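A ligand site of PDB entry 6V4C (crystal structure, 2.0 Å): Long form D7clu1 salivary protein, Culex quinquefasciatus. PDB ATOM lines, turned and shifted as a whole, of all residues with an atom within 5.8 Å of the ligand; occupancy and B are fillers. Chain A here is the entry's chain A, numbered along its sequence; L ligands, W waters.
The backbone carbonyl oxygen (O) of Lys 144 lies within hydrogen-bond range of a nitrogen (N3) of the ligand (2.9 Å).
A nitrogen (N4) of the ligand is in hydrogen-bond range of the side-chain amino group of Lys 144 (3.0 Å).
NH1 of Arg 133 is in salt-bridge range of O3 of the ligand (3.1 Å).
The side-chain hydroxyl (OH) of Tyr 137 sits at hydrogen-bond distance from a nitrogen (N2) of the ligand (2.9 Å).
N5 of the ligand sits at hydrogen-bond distance from N of Tyr 266 (3.0 Å).
The side-chain hydroxyl (OG) of Ser 267 is in hydrogen-bond range of an oxygen (O9) of the ligand (2.4 Å).
The side-chain amide nitrogen (ND2) of Asn 265 lies within hydrogen-bond range of an oxygen (O7) of the ligand (3.3 Å).
N of Ser 267 lies within hydrogen-bond range of O10 of the ligand, at 3.5 Å.
The backbone NH (N) of Glu 9 sits at hydrogen-bond distance from the side-chain hydroxyl (OH) of Tyr 137 (3.4 Å).
N of Ser 267 sits close to OD1 of Asn 265, at 3.1 Å.
The side-chain hydroxyl (OH) of Tyr 266 lies within hydrogen-bond range of the side-chain carboxylate (OE2) of Glu 9.
N of Gly 147 is in hydrogen-bond range of O of Glu 264 (2.8 Å).
NZ of Lys 144 lies within hydrogen-bond range of O of Ser 263, 2.9 Å away.
The guanidinium group (NE) of Arg 133 lies within salt-bridge range of the side-chain carboxylate (OD1) of Asp 134 (3.2 Å).
The backbone carbonyl oxygen (O) of Ile 148 lies within hydrogen-bond range of the side-chain amino group (NZ) of Lys 144 (2.9 Å).
N3 of the ligand sits close to N of Lys 146 (3.5 Å).
Residues that only touch the ligand: Glu 9 (3.4 Å), Ala 12 (3.5 Å), Pro 145 (3.4 Å), Ser 263 (3.5 Å) and Glu 264 (3.7 Å).
Within 4 Å of the ligand: Glu 9, Ala 12, Arg 133, Tyr 137, Lys 144, Pro 145, Lys 146, Ser 263, Glu 264, Asn 265, Tyr 266 and Ser 267.
Water W1 lies within hydrogen-bond range of an oxygen (O10) of the ligand, the side-chain carboxylate of Glu 15 and the backbone carbonyl oxygen of Ala 12.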
ATOM      1  N   PRO A   8       1.861  -6.933   1.245  1.00  0.00           N
ATOM      2  CA  PRO A   8       2.176  -7.655   2.490  1.00  0.00           C
ATOM      3  C   PRO A   8       1.148  -7.478   3.590  1.00  0.00           C
ATOM      4  O   PRO A   8       0.991  -8.383   4.425  1.00  0.00           O
ATOM      5  CB  PRO A   8       3.549  -7.080   2.912  1.00  0.00           C
ATOM      6  CG  PRO A   8       4.082  -6.420   1.687  1.00  0.00           C
ATOM      7  CD  PRO A   8       2.886  -5.916   0.944  1.00  0.00           C
ATOM      8  N   GLU A   9       0.436  -6.340   3.618  1.00  0.00           N
ATOM      9  CA  GLU A   9      -0.614  -6.147   4.622  1.00  0.00           C
ATOM     10  C   GLU A   9      -1.799  -7.063   4.367  1.00  0.00           C
ATOM     11  O   GLU A   9      -2.359  -7.648   5.304  1.00  0.00           O
ATOM     12  CB  GLU A   9      -1.051  -4.681   4.647  1.00  0.00           C
ATOM     13  CG  GLU A   9      -2.111  -4.341   5.708  1.00  0.00           C
ATOM     14  CD  GLU A   9      -3.542  -4.550   5.223  1.00  0.00           C
ATOM     15  OE1 GLU A   9      -3.754  -4.723   4.007  1.00  0.00           O
ATOM     16  OE2 GLU A   9      -4.468  -4.523   6.071  1.00  0.00           O
ATOM     17  N   ALA A  12      -0.758 -10.635   5.375  1.00  0.00           N
ATOM     18  CA  ALA A  12      -0.710 -10.766   6.827  1.00  0.00           C
ATOM     19  C   ALA A  12      -2.116 -10.779   7.427  1.00  0.00           C
ATOM     20  O   ALA A  12      -2.389 -11.530   8.379  1.00  0.00           O
ATOM     21  CB  ALA A  12       0.137  -9.645   7.433  1.00  0.00           C
ATOM     22  N   GLU A  15      -3.515 -14.315   6.579  1.00  0.00           N
ATOM     23  CA  GLU A  15      -2.837 -15.354   7.356  1.00  0.00           C
ATOM     24  C   GLU A  15      -3.333 -15.375   8.798  1.00  0.00           C
ATOM     25  O   GLU A  15      -3.628 -16.434   9.343  1.00  0.00           O
ATOM     26  CB  GLU A  15      -1.317 -15.145   7.321  1.00  0.00           C
ATOM     27  CG  GLU A  15      -0.546 -16.194   8.125  1.00  0.00           C
ATOM     28  CD  GLU A  15       0.884 -15.786   8.415  1.00  0.00           C
ATOM     29  OE1 GLU A  15       1.811 -16.434   7.870  1.00  0.00           O
ATOM     30  OE2 GLU A  15       1.080 -14.827   9.194  1.00  0.00           O
ATOM     31  N   ALA A  16      -3.418 -14.191   9.421  1.00  0.00           N
ATOM     32  CA  ALA A  16      -3.865 -14.116  10.812  1.00  0.00           C
ATOM     33  C   ALA A  16      -5.293 -14.613  10.963  1.00  0.00           C
ATOM     34  O   ALA A  16      -5.624 -15.269  11.964  1.00  0.00           O
ATOM     35  CB  ALA A  16      -3.726 -12.685  11.315  1.00  0.00           C
ATOM     36  N   MET A  34       3.220 -19.294  12.388  1.00  0.00           N
ATOM     37  CA  MET A  34       3.845 -18.014  12.057  1.00  0.00           C
ATOM     38  C   MET A  34       5.254 -18.221  11.499  1.00  0.00           C
ATOM     39  O   MET A  34       5.677 -17.500  10.582  1.00  0.00           O
ATOM     40  CB  MET A  34       3.905 -17.116  13.293  1.00  0.00           C
ATOM     41  CG  MET A  34       2.557 -16.875  13.953  1.00  0.00           C
ATOM     42  SD  MET A  34       2.634 -15.663  15.280  1.00  0.00           S
ATOM     43  CE  MET A  34       1.410 -16.301  16.399  1.00  0.00           C
ATOM     44  N   LEU A 128       5.485 -12.467   3.299  1.00  0.00           N
ATOM     45  CA  LEU A 128       5.474 -12.719   4.733  1.00  0.00           C
ATOM     46  C   LEU A 128       6.863 -12.730   5.340  1.00  0.00           C
ATOM     47  O   LEU A 128       6.995 -12.607   6.567  1.00  0.00           O
ATOM     48  CB  LEU A 128       4.757 -14.032   5.040  1.00  0.00           C
ATOM     49  CG  LEU A 128       3.246 -14.045   4.748  1.00  0.00           C
ATOM     50  CD1 LEU A 128       2.688 -15.446   4.893  1.00  0.00           C
ATOM     51  CD2 LEU A 128       2.516 -13.081   5.680  1.00  0.00           C
ATOM     52  N   SER A 130      10.142 -11.291   6.720  1.00  0.00           N
ATOM     53  CA  SER A 130      10.244 -10.010   7.419  1.00  0.00           C
ATOM     54  C   SER A 130      10.995  -8.972   6.597  1.00  0.00           C
ATOM     55  O   SER A 130      10.599  -7.798   6.565  1.00  0.00           O
ATOM     56  CB  SER A 130      10.908 -10.212   8.781  1.00  0.00           C
ATOM     57  OG  SER A 130      12.234 -10.671   8.632  1.00  0.00           O
ATOM     58  N   ARG A 133       8.805  -7.917   3.437  1.00  0.00           N
ATOM     59  CA  ARG A 133       7.652  -7.143   3.950  1.00  0.00           C
ATOM     60  C   ARG A 133       8.071  -5.735   4.332  1.00  0.00           C
ATOM     61  O   ARG A 133       7.547  -4.878   3.854  1.00  0.00           O
ATOM     62  CB  ARG A 133       7.083  -7.904   5.115  1.00  0.00           C
ATOM     63  CG  ARG A 133       5.948  -7.256   5.868  1.00  0.00           C
ATOM     64  CD  ARG A 133       5.617  -7.830   7.191  1.00  0.00           C
ATOM     65  NE  ARG A 133       6.642  -7.561   8.102  1.00  0.00           N
ATOM     66  CZ  ARG A 133       7.035  -8.290   9.055  1.00  0.00           C
ATOM     67  NH1 ARG A 133       6.473  -9.415   9.315  1.00  0.00           N
ATOM     68  NH2 ARG A 133       8.006  -7.888   9.787  1.00  0.00           N
ATOM     69  N   ASP A 134       9.107  -5.645   5.127  1.00  0.00           N
ATOM     70  CA  ASP A 134       9.474  -4.335   5.649  1.00  0.00           C
ATOM     71  C   ASP A 134      10.020  -3.419   4.566  1.00  0.00           C
ATOM     72  O   ASP A 134       9.769  -2.213   4.595  1.00  0.00           O
ATOM     73  CB  ASP A 134      10.453  -4.488   6.808  1.00  0.00           C
ATOM     74  CG  ASP A 134       9.798  -5.063   8.051  1.00  0.00           C
ATOM     75  OD1 ASP A 134       8.551  -4.970   8.159  1.00  0.00           O
ATOM     76  OD2 ASP A 134      10.519  -5.604   8.916  1.00  0.00           O
ATOM     77  N   TYR A 137       7.001  -2.045   2.736  1.00  0.00           N
ATOM     78  CA  TYR A 137       6.367  -1.004   3.543  1.00  0.00           C
ATOM     79  C   TYR A 137       7.134   0.305   3.446  1.00  0.00           C
ATOM     80  O   TYR A 137       6.535   1.377   3.273  1.00  0.00           O
ATOM     81  CB  TYR A 137       6.264  -1.442   5.008  1.00  0.00           C
ATOM     82  CG  TYR A 137       5.242  -2.527   5.296  1.00  0.00           C
ATOM     83  CD1 TYR A 137       4.229  -2.822   4.398  1.00  0.00           C
ATOM     84  CD2 TYR A 137       5.294  -3.232   6.487  1.00  0.00           C
ATOM     85  CE1 TYR A 137       3.299  -3.815   4.669  1.00  0.00           C
ATOM     86  CE2 TYR A 137       4.368  -4.219   6.771  1.00  0.00           C
ATOM     87  CZ  TYR A 137       3.374  -4.516   5.859  1.00  0.00           C
ATOM     88  OH  TYR A 137       2.466  -5.499   6.151  1.00  0.00           O
ATOM     89  N   LYS A 144      -0.697   0.327   4.759  1.00  0.00           N
ATOM     90  CA  LYS A 144      -0.642   0.392   6.217  1.00  0.00           C
ATOM     91  C   LYS A 144       0.376  -0.613   6.739  1.00  0.00           C
ATOM     92  O   LYS A 144       0.172  -1.818   6.566  1.00  0.00           O
ATOM     93  CB  LYS A 144      -2.017   0.082   6.812  1.00  0.00           C
ATOM     94  CG  LYS A 144      -2.080   0.330   8.321  1.00  0.00           C
ATOM     95  CD  LYS A 144      -3.209  -0.431   8.993  1.00  0.00           C
ATOM     96  CE  LYS A 144      -2.817  -1.862   9.327  1.00  0.00           C
ATOM     97  NZ  LYS A 144      -1.758  -1.945  10.378  1.00  0.00           N
ATOM     98  N   PRO A 145       1.470  -0.169   7.359  1.00  0.00           N
ATOM     99  CA  PRO A 145       2.460  -1.130   7.866  1.00  0.00           C
ATOM    100  C   PRO A 145       2.061  -1.629   9.248  1.00  0.00           C
ATOM    101  O   PRO A 145       1.058  -1.160   9.806  1.00  0.00           O
ATOM    102  CB  PRO A 145       3.739  -0.301   7.927  1.00  0.00           C
ATOM    103  CG  PRO A 145       3.233   1.081   8.287  1.00  0.00           C
ATOM    104  CD  PRO A 145       1.870   1.228   7.631  1.00  0.00           C
ATOM    105  N   LYS A 146       2.820  -2.546   9.824  1.00  0.00           N
ATOM    106  CA  LYS A 146       2.515  -2.937  11.200  1.00  0.00           C
ATOM    107  C   LYS A 146       2.990  -1.842  12.159  1.00  0.00           C
ATOM    108  O   LYS A 146       3.853  -1.032  11.825  1.00  0.00           O
ATOM    109  CB  LYS A 146       3.120  -4.303  11.540  1.00  0.00           C
ATOM    110  CG  LYS A 146       4.446  -4.286  12.280  1.00  0.00           C
ATOM    111  CD  LYS A 146       4.833  -5.708  12.702  1.00  0.00           C
ATOM    112  CE  LYS A 146       6.240  -5.764  13.295  1.00  0.00           C
ATOM    113  NZ  LYS A 146       7.288  -5.469  12.278  1.00  0.00           N
ATOM    114  N   GLY A 147       2.374  -1.796  13.326  1.00  0.00           N
ATOM    115  CA  GLY A 147       2.718  -0.820  14.334  1.00  0.00           C
ATOM    116  C   GLY A 147       1.836   0.417  14.378  1.00  0.00           C
ATOM    117  O   GLY A 147       1.950   1.205  15.314  1.00  0.00           O
ATOM    118  N   ILE A 148       0.970   0.610  13.378  1.00  0.00           N
ATOM    119  CA  ILE A 148       0.016   1.710  13.367  1.00  0.00           C
ATOM    120  C   ILE A 148      -1.368   1.137  13.136  1.00  0.00           C
ATOM    121  O   ILE A 148      -1.542   0.207  12.336  1.00  0.00           O
ATOM    122  CB  ILE A 148       0.387   2.779  12.304  1.00  0.00           C
ATOM    123  CG1 ILE A 148      -0.537   3.990  12.414  1.00  0.00           C
ATOM    124  CG2 ILE A 148       0.337   2.189  10.905  1.00  0.00           C
ATOM    125  CD1 ILE A 148      -0.153   5.138  11.507  1.00  0.00           C
ATOM    126  N   ARG A 262      -6.137  -4.392  17.829  1.00  0.00           N
ATOM    127  CA  ARG A 262      -5.620  -5.562  17.127  1.00  0.00           C
ATOM    128  C   ARG A 262      -5.027  -5.229  15.772  1.00  0.00           C
ATOM    129  O   ARG A 262      -4.198  -5.983  15.267  1.00  0.00           O
ATOM    130  CB  ARG A 262      -6.729  -6.605  16.969  1.00  0.00           C
ATOM    131  CG  ARG A 262      -7.259  -7.178  18.285  1.00  0.00           C
ATOM    132  CD  ARG A 262      -8.743  -7.498  18.174  1.00  0.00           C
ATOM    133  NE  ARG A 262      -9.029  -8.476  17.137  1.00  0.00           N
ATOM    134  CZ  ARG A 262     -10.214  -8.612  16.546  1.00  0.00           C
ATOM    135  NH1 ARG A 262     -11.227  -7.810  16.866  1.00  0.00           N
ATOM    136  NH2 ARG A 262     -10.375  -9.529  15.599  1.00  0.00           N
ATOM    137  N   SER A 263      -5.438  -4.113  15.162  1.00  0.00           N
ATOM    138  CA  SER A 263      -4.995  -3.768  13.810  1.00  0.00           C
ATOM    139  C   SER A 263      -3.550  -3.318  13.761  1.00  0.00           C
ATOM    140  O   SER A 263      -2.987  -3.241  12.660  1.00  0.00           O
ATOM    141  CB  SER A 263      -5.906  -2.695  13.195  1.00  0.00           C
ATOM    142  OG  SER A 263      -5.660  -1.409  13.757  1.00  0.00           O
ATOM    143  N   GLU A 264      -2.936  -3.004  14.906  1.00  0.00           N
ATOM    144  CA  GLU A 264      -1.516  -2.631  14.890  1.00  0.00           C
ATOM    145  C   GLU A 264      -0.629  -3.840  14.623  1.00  0.00           C
ATOM    146  O   GLU A 264       0.465  -3.697  14.063  1.00  0.00           O
ATOM    147  CB  GLU A 264      -1.131  -1.950  16.198  1.00  0.00           C
ATOM    148  CG  GLU A 264      -1.836  -0.621  16.429  1.00  0.00           C
ATOM    149  CD  GLU A 264      -1.208   0.188  17.544  1.00  0.00           C
ATOM    150  OE1 GLU A 264      -0.293  -0.337  18.224  1.00  0.00           O
ATOM    151  OE2 GLU A 264      -1.620   1.356  17.746  1.00  0.00           O
ATOM    152  N   ASN A 265      -1.090  -5.041  14.989  1.00  0.00           N
ATOM    153  CA  ASN A 265      -0.349  -6.265  14.735  1.00  0.00           C
ATOM    154  C   ASN A 265      -1.379  -7.387  14.684  1.00  0.00           C
ATOM    155  O   ASN A 265      -1.920  -7.785  15.715  1.00  0.00           O
ATOM    156  CB  ASN A 265       0.689  -6.520  15.825  1.00  0.00           C
ATOM    157  CG  ASN A 265       1.611  -7.682  15.493  1.00  0.00           C
ATOM    158  OD1 ASN A 265       1.165  -8.726  15.028  1.00  0.00           O
ATOM    159  ND2 ASN A 265       2.901  -7.486  15.728  1.00  0.00           N
ATOM    160  N   TYR A 266      -1.623  -7.917  13.472  1.00  0.00           N
ATOM    161  CA  TYR A 266      -2.726  -8.845  13.272  1.00  0.00           C
ATOM    162  C   TYR A 266      -2.574 -10.153  14.051  1.00  0.00           C
ATOM    163  O   TYR A 266      -3.564 -10.870  14.216  1.00  0.00           O
ATOM    164  CB  TYR A 266      -2.913  -9.135  11.779  1.00  0.00           C
ATOM    165  CG  TYR A 266      -3.295  -7.914  10.969  1.00  0.00           C
ATOM    166  CD1 TYR A 266      -4.155  -6.948  11.479  1.00  0.00           C
ATOM    167  CD2 TYR A 266      -2.779  -7.727   9.686  1.00  0.00           C
ATOM    168  CE1 TYR A 266      -4.500  -5.836  10.740  1.00  0.00           C
ATOM    169  CE2 TYR A 266      -3.121  -6.608   8.935  1.00  0.00           C
ATOM    170  CZ  TYR A 266      -3.977  -5.662   9.477  1.00  0.00           C
ATOM    171  OH  TYR A 266      -4.317  -4.562   8.733  1.00  0.00           O
ATOM    172  N   SER A 267      -1.374 -10.460  14.534  1.00  0.00           N
ATOM    173  CA  SER A 267      -1.143 -11.660  15.344  1.00  0.00           C
ATOM    174  C   SER A 267      -1.471 -11.453  16.815  1.00  0.00           C
ATOM    175  O   SER A 267      -1.137 -12.325  17.630  1.00  0.00           O
ATOM    176  CB  SER A 267       0.319 -12.098  15.200  1.00  0.00           C
ATOM    177  OG  SER A 267       0.708 -12.188  13.852  1.00  0.00           O
ATOM    178  N   ARG A 271      -0.907 -14.504  20.419  1.00  0.00           N
ATOM    179  CA  ARG A 271       0.015 -14.652  21.525  1.00  0.00           C
ATOM    180  C   ARG A 271      -0.819 -14.820  22.749  1.00  0.00           C
ATOM    181  O   ARG A 271      -1.770 -14.220  22.869  1.00  0.00           O
ATOM    182  CB  ARG A 271       0.864 -13.456  21.799  1.00  0.00           C
ATOM    183  CG  ARG A 271       1.291 -12.844  20.513  1.00  0.00           C
ATOM    184  CD  ARG A 271       2.605 -13.318  20.237  1.00  0.00           C
ATOM    185  NE  ARG A 271       2.536 -12.916  18.893  1.00  0.00           N
ATOM    186  CZ  ARG A 271       2.385 -11.710  18.431  1.00  0.00           C
ATOM    187  NH1 ARG A 271       2.236 -10.673  19.179  1.00  0.00           N
ATOM    188  NH2 ARG A 271       2.428 -11.517  17.178  1.00  0.00           N
HETATM  189  P1  LIG L   1       8.484 -10.091  12.889  1.00  0.00           P
HETATM  190  O1  LIG L   1       9.578  -9.273  12.725  1.00  0.00           O
HETATM  191  O2  LIG L   1       8.640 -11.074  13.889  1.00  0.00           O
HETATM  192  O3  LIG L   1       8.093 -10.663  11.709  1.00  0.00           O
HETATM  193  P2  LIG L   1       6.610  -9.399  15.003  1.00  0.00           P
HETATM  194  O4  LIG L   1       7.047  -8.562  16.154  1.00  0.00           O
HETATM  195  O5  LIG L   1       6.657 -10.763  15.366  1.00  0.00           O
HETATM  196  O6  LIG L   1       7.463  -9.191  13.730  1.00  0.00           O
HETATM  197  O7  LIG L   1       5.329  -9.150  14.209  1.00  0.00           O
HETATM  198  C1  LIG L   1       5.013  -9.879  13.041  1.00  0.00           C
HETATM  199  C2  LIG L   1       3.530  -9.851  12.762  1.00  0.00           C
HETATM  200  O8  LIG L   1       3.145  -8.706  12.041  1.00  0.00           O
HETATM  201  C3  LIG L   1       2.981 -10.890  11.809  1.00  0.00           C
HETATM  202  O9  LIG L   1       2.695 -12.101  12.437  1.00  0.00           O
HETATM  203  C4  LIG L   1       1.768 -10.253  11.146  1.00  0.00           C
HETATM  204  O10 LIG L   1       0.614 -10.717  11.698  1.00  0.00           O
HETATM  205  C5  LIG L   1       1.868  -8.829  11.585  1.00  0.00           C
HETATM  206  N1  LIG L   1       1.683  -7.852  10.550  1.00  0.00           N
HETATM  207  C6  LIG L   1       2.379  -7.793   9.438  1.00  0.00           C
HETATM  208  N2  LIG L   1       2.077  -6.817   8.691  1.00  0.00           N
HETATM  209  C7  LIG L   1       1.098  -6.173   9.337  1.00  0.00           C
HETATM  210  C8  LIG L   1       0.345  -5.042   9.060  1.00  0.00           C
HETATM  211  N3  LIG L   1       0.448  -4.322   7.998  1.00  0.00           N
HETATM  212  N4  LIG L   1      -0.568  -4.672   9.932  1.00  0.00           N
HETATM  213  C9  LIG L   1      -0.720  -5.385  11.002  1.00  0.00           C
HETATM  214  N5  LIG L   1      -0.077  -6.424  11.372  1.00  0.00           N
HETATM  215  C10 LIG L   1       0.837  -6.803  10.503  1.00  0.00           C
HETATM  216  O   HOH W   1      -0.250 -12.509  10.055  1.00  0.00           O
HETATM  217  O   HOH W   2       4.030 -10.410   8.118  1.00  0.00           O
